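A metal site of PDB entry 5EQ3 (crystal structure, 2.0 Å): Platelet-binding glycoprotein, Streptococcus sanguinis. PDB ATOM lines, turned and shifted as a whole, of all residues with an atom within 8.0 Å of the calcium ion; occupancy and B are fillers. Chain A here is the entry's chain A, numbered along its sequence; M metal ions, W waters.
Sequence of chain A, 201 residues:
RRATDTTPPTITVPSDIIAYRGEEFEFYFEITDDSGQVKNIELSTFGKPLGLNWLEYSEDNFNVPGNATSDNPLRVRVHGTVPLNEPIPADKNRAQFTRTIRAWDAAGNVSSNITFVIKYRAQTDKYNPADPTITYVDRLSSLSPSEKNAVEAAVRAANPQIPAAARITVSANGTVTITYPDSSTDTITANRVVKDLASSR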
ATOM      1  N   ALA A 122     -23.101 -12.006   8.055  1.00  0.00           N
ATOM      2  CA  ALA A 122     -23.132 -13.433   8.360  1.00  0.00           C
ATOM      3  C   ALA A 122     -23.882 -13.699   9.659  1.00  0.00           C
ATOM      4  O   ALA A 122     -23.871 -12.886  10.588  1.00  0.00           O
ATOM      5  CB  ALA A 122     -21.716 -13.968   8.437  1.00  0.00           C
ATOM      6  N   GLN A 123     -24.536 -14.854   9.735  1.00  0.00           N
ATOM      7  CA  GLN A 123     -25.350 -15.179  10.895  1.00  0.00           C
ATOM      8  C   GLN A 123     -24.569 -15.166  12.207  1.00  0.00           C
ATOM      9  O   GLN A 123     -25.115 -14.837  13.238  1.00  0.00           O
ATOM     10  CB  GLN A 123     -26.051 -16.523  10.703  1.00  0.00           C
ATOM     11  CG  GLN A 123     -27.401 -16.355  10.056  1.00  0.00           C
ATOM     12  CD  GLN A 123     -28.028 -17.663   9.643  1.00  0.00           C
ATOM     13  OE1 GLN A 123     -27.411 -18.454   8.926  1.00  0.00           O
ATOM     14  NE2 GLN A 123     -29.248 -17.894  10.087  1.00  0.00           N
ATOM     15  N   THR A 124     -23.285 -15.469  12.168  1.00  0.00           N
ATOM     16  CA  THR A 124     -22.554 -15.529  13.419  1.00  0.00           C
ATOM     17  C   THR A 124     -22.360 -14.137  14.001  1.00  0.00           C
ATOM     18  O   THR A 124     -22.122 -14.008  15.207  1.00  0.00           O
ATOM     19  CB  THR A 124     -21.167 -16.216  13.272  1.00  0.00           C
ATOM     20  OG1 THR A 124     -20.501 -16.177  14.543  1.00  0.00           O
ATOM     21  CG2 THR A 124     -20.310 -15.547  12.192  1.00  0.00           C
ATOM     22  N   ASP A 125     -22.482 -13.100  13.170  1.00  0.00           N
ATOM     23  CA  ASP A 125     -22.404 -11.741  13.688  1.00  0.00           C
ATOM     24  C   ASP A 125     -23.581 -11.465  14.611  1.00  0.00           C
ATOM     25  O   ASP A 125     -23.470 -10.687  15.567  1.00  0.00           O
ATOM     26  CB  ASP A 125     -22.346 -10.720  12.548  1.00  0.00           C
ATOM     27  CG  ASP A 125     -21.017 -10.739  11.837  1.00  0.00           C
ATOM     28  OD1 ASP A 125     -20.236 -11.687  12.055  1.00  0.00           O
ATOM     29  OD2 ASP A 125     -20.748  -9.806  11.047  1.00  0.00           O
ATOM     30  N   LYS A 126     -24.710 -12.103  14.323  1.00  0.00           N
ATOM     31  CA  LYS A 126     -25.900 -11.965  15.144  1.00  0.00           C
ATOM     32  C   LYS A 126     -25.815 -12.776  16.430  1.00  0.00           C
ATOM     33  O   LYS A 126     -26.337 -12.360  17.478  1.00  0.00           O
ATOM     34  CB  LYS A 126     -27.132 -12.404  14.358  1.00  0.00           C
ATOM     35  CG  LYS A 126     -28.396 -12.437  15.179  1.00  0.00           C
ATOM     36  CD  LYS A 126     -29.610 -12.666  14.327  1.00  0.00           C
ATOM     37  CE  LYS A 126     -30.820 -12.869  15.183  1.00  0.00           C
ATOM     38  NZ  LYS A 126     -32.026 -13.139  14.345  1.00  0.00           N
ATOM     39  N   TYR A 127     -25.176 -13.940  16.353  1.00  0.00           N
ATOM     40  CA  TYR A 127     -25.252 -14.907  17.450  1.00  0.00           C
ATOM     41  C   TYR A 127     -23.979 -14.989  18.286  1.00  0.00           C
ATOM     42  O   TYR A 127     -22.864 -15.044  17.745  1.00  0.00           O
ATOM     43  CB  TYR A 127     -25.631 -16.285  16.901  1.00  0.00           C
ATOM     44  CG  TYR A 127     -26.989 -16.287  16.236  1.00  0.00           C
ATOM     45  CD1 TYR A 127     -28.150 -16.171  16.987  1.00  0.00           C
ATOM     46  CD2 TYR A 127     -27.111 -16.366  14.854  1.00  0.00           C
ATOM     47  CE1 TYR A 127     -29.402 -16.159  16.379  1.00  0.00           C
ATOM     48  CE2 TYR A 127     -28.356 -16.355  14.238  1.00  0.00           C
ATOM     49  CZ  TYR A 127     -29.498 -16.252  15.011  1.00  0.00           C
ATOM     50  OH  TYR A 127     -30.743 -16.240  14.410  1.00  0.00           O
ATOM     51  N   ASN A 128     -24.171 -14.987  19.599  1.00  0.00           N
ATOM     52  CA  ASN A 128     -23.089 -15.107  20.558  1.00  0.00           C
ATOM     53  C   ASN A 128     -23.382 -16.244  21.541  1.00  0.00           C
ATOM     54  O   ASN A 128     -24.155 -16.084  22.492  1.00  0.00           O
ATOM     55  CB  ASN A 128     -22.886 -13.791  21.309  1.00  0.00           C
ATOM     56  CG  ASN A 128     -21.622 -13.781  22.152  1.00  0.00           C
ATOM     57  OD1 ASN A 128     -20.647 -14.459  21.834  1.00  0.00           O
ATOM     58  ND2 ASN A 128     -21.640 -13.009  23.235  1.00  0.00           N
ATOM     59  N   PRO A 129     -22.771 -17.420  21.299  1.00  0.00           N
ATOM     60  CA  PRO A 129     -23.072 -18.641  22.074  1.00  0.00           C
ATOM     61  C   PRO A 129     -22.646 -18.554  23.537  1.00  0.00           C
ATOM     62  O   PRO A 129     -21.491 -18.253  23.821  1.00  0.00           O
ATOM     63  CB  PRO A 129     -22.285 -19.717  21.341  1.00  0.00           C
ATOM     64  CG  PRO A 129     -21.197 -18.987  20.629  1.00  0.00           C
ATOM     65  CD  PRO A 129     -21.768 -17.659  20.253  1.00  0.00           C
ATOM     66  N   ILE A 162     -30.343 -19.655  19.463  1.00  0.00           N
ATOM     67  CA  ILE A 162     -29.624 -20.043  18.257  1.00  0.00           C
ATOM     68  C   ILE A 162     -30.565 -20.811  17.340  1.00  0.00           C
ATOM     69  O   ILE A 162     -31.452 -21.522  17.822  1.00  0.00           O
ATOM     70  CB  ILE A 162     -28.362 -20.868  18.618  1.00  0.00           C
ATOM     71  CG1 ILE A 162     -27.111 -19.986  18.591  1.00  0.00           C
ATOM     72  CG2 ILE A 162     -28.195 -22.099  17.726  1.00  0.00           C
ATOM     73  CD1 ILE A 162     -25.847 -20.712  19.032  1.00  0.00           C
ATOM     74  N   ILE A 178     -20.085 -24.499  16.072  1.00  0.00           N
ATOM     75  CA  ILE A 178     -21.486 -24.211  15.743  1.00  0.00           C
ATOM     76  C   ILE A 178     -21.532 -23.634  14.348  1.00  0.00           C
ATOM     77  O   ILE A 178     -20.967 -22.573  14.095  1.00  0.00           O
ATOM     78  CB  ILE A 178     -22.116 -23.203  16.717  1.00  0.00           C
ATOM     79  CG1 ILE A 178     -22.132 -23.752  18.144  1.00  0.00           C
ATOM     80  CG2 ILE A 178     -23.543 -22.838  16.261  1.00  0.00           C
ATOM     81  CD1 ILE A 178     -22.575 -22.761  19.179  1.00  0.00           C
ATOM     82  N   TYR A 180     -23.842 -22.162  11.582  1.00  0.00           N
ATOM     83  CA  TYR A 180     -25.122 -21.577  11.230  1.00  0.00           C
ATOM     84  C   TYR A 180     -25.577 -21.954   9.830  1.00  0.00           C
ATOM     85  O   TYR A 180     -24.760 -22.365   9.018  1.00  0.00           O
ATOM     86  CB  TYR A 180     -25.010 -20.052  11.391  1.00  0.00           C
ATOM     87  CG  TYR A 180     -24.605 -19.719  12.802  1.00  0.00           C
ATOM     88  CD1 TYR A 180     -25.508 -19.856  13.839  1.00  0.00           C
ATOM     89  CD2 TYR A 180     -23.312 -19.345  13.094  1.00  0.00           C
ATOM     90  CE1 TYR A 180     -25.140 -19.576  15.140  1.00  0.00           C
ATOM     91  CE2 TYR A 180     -22.936 -19.066  14.388  1.00  0.00           C
ATOM     92  CZ  TYR A 180     -23.857 -19.180  15.404  1.00  0.00           C
ATOM     93  OH  TYR A 180     -23.474 -18.902  16.691  1.00  0.00           O
ATOM     94  N   SER A 184     -21.549 -19.760   8.256  1.00  0.00           N
ATOM     95  CA  SER A 184     -20.645 -19.016   9.135  1.00  0.00           C
ATOM     96  C   SER A 184     -20.637 -19.738  10.475  1.00  0.00           C
ATOM     97  O   SER A 184     -21.580 -20.447  10.806  1.00  0.00           O
ATOM     98  CB  SER A 184     -21.069 -17.550   9.294  1.00  0.00           C
ATOM     99  OG  SER A 184     -22.351 -17.443   9.882  1.00  0.00           O
ATOM    100  N   THR A 185     -19.564 -19.579  11.254  1.00  0.00           N
ATOM    101  CA  THR A 185     -19.366 -20.444  12.418  1.00  0.00           C
ATOM    102  C   THR A 185     -19.002 -19.687  13.685  1.00  0.00           C
ATOM    103  O   THR A 185     -18.544 -18.537  13.647  1.00  0.00           O
ATOM    104  CB  THR A 185     -18.263 -21.483  12.150  1.00  0.00           C
ATOM    105  OG1 THR A 185     -17.012 -20.828  11.942  1.00  0.00           O
ATOM    106  CG2 THR A 185     -18.583 -22.327  10.912  1.00  0.00           C
ATOM    107  N   ASP A 186     -19.238 -20.341  14.821  1.00  0.00           N
ATOM    108  CA  ASP A 186     -18.693 -19.923  16.106  1.00  0.00           C
ATOM    109  C   ASP A 186     -17.953 -21.138  16.686  1.00  0.00           C
ATOM    110  O   ASP A 186     -18.175 -22.267  16.234  1.00  0.00           O
ATOM    111  CB  ASP A 186     -19.778 -19.428  17.060  1.00  0.00           C
ATOM    112  CG  ASP A 186     -20.178 -17.945  16.824  1.00  0.00           C
ATOM    113  OD1 ASP A 186     -19.311 -17.105  16.513  1.00  0.00           O
ATOM    114  OD2 ASP A 186     -21.370 -17.607  16.975  1.00  0.00           O
ATOM    115  N   THR A 187     -17.066 -20.908  17.639  1.00  0.00           N
ATOM    116  CA  THR A 187     -16.282 -22.008  18.223  1.00  0.00           C
ATOM    117  C   THR A 187     -16.236 -21.851  19.737  1.00  0.00           C
ATOM    118  O   THR A 187     -16.245 -20.723  20.246  1.00  0.00           O
ATOM    119  CB  THR A 187     -14.851 -22.064  17.644  1.00  0.00           C
ATOM    120  OG1 THR A 187     -14.931 -22.269  16.233  1.00  0.00           O
ATOM    121  CG2 THR A 187     -14.054 -23.216  18.249  1.00  0.00           C
HETATM  122 CA    CA M   1     -20.859 -15.308  16.735  1.00  0.00          CA
HETATM  123  O   HOH W   1     -18.694 -14.661  15.983  1.00  0.00           O
HETATM  124  O   HOH W   2     -20.547 -13.303  18.000  1.00  0.00           O
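OH of Tyr 127 sits at hydrogen-bond distance from NZ of Lys 126.
OH of Tyr 180 lies close to OD2 of Asp 186.
The side-chain hydroxyl (OG1) of Thr 124 sits close to the backbone carbonyl oxygen (O) of Thr 185 (3.2 Å).
O of Ile 178 sits at hydrogen-bond distance from N of Asp 186 (2.9 Å).
The backbone NH (N) of Thr 124 lies within hydrogen-bond range of the side-chain hydroxyl (OG) of Ser 184 (3.2 Å).
Three residues have an atom within 4 Å of the calcium ion: Thr 124, Tyr 127 and Asp 186.
The nearest printed residue that does not touch the calcium ion is Pro 129 (4.3 Å).
The calcium ion is bound by the backbone carbonyl oxygen (O) of Tyr 127 (2.3 Å), the side-chain carboxylate (OD2) of Asp 186 (2.4 Å), the backbone carbonyl oxygen (O) of Thr 124 (2.4 Å), water W1 (2.4 Å), the side-chain carboxylate (OD1) of Asp 186 (2.4 Å), the side-chain hydroxyl (OG1) of Thr 124 (2.4 Å) and water W2 (2.4 Å).
The calcium ion has seven donor atoms within binding distance.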
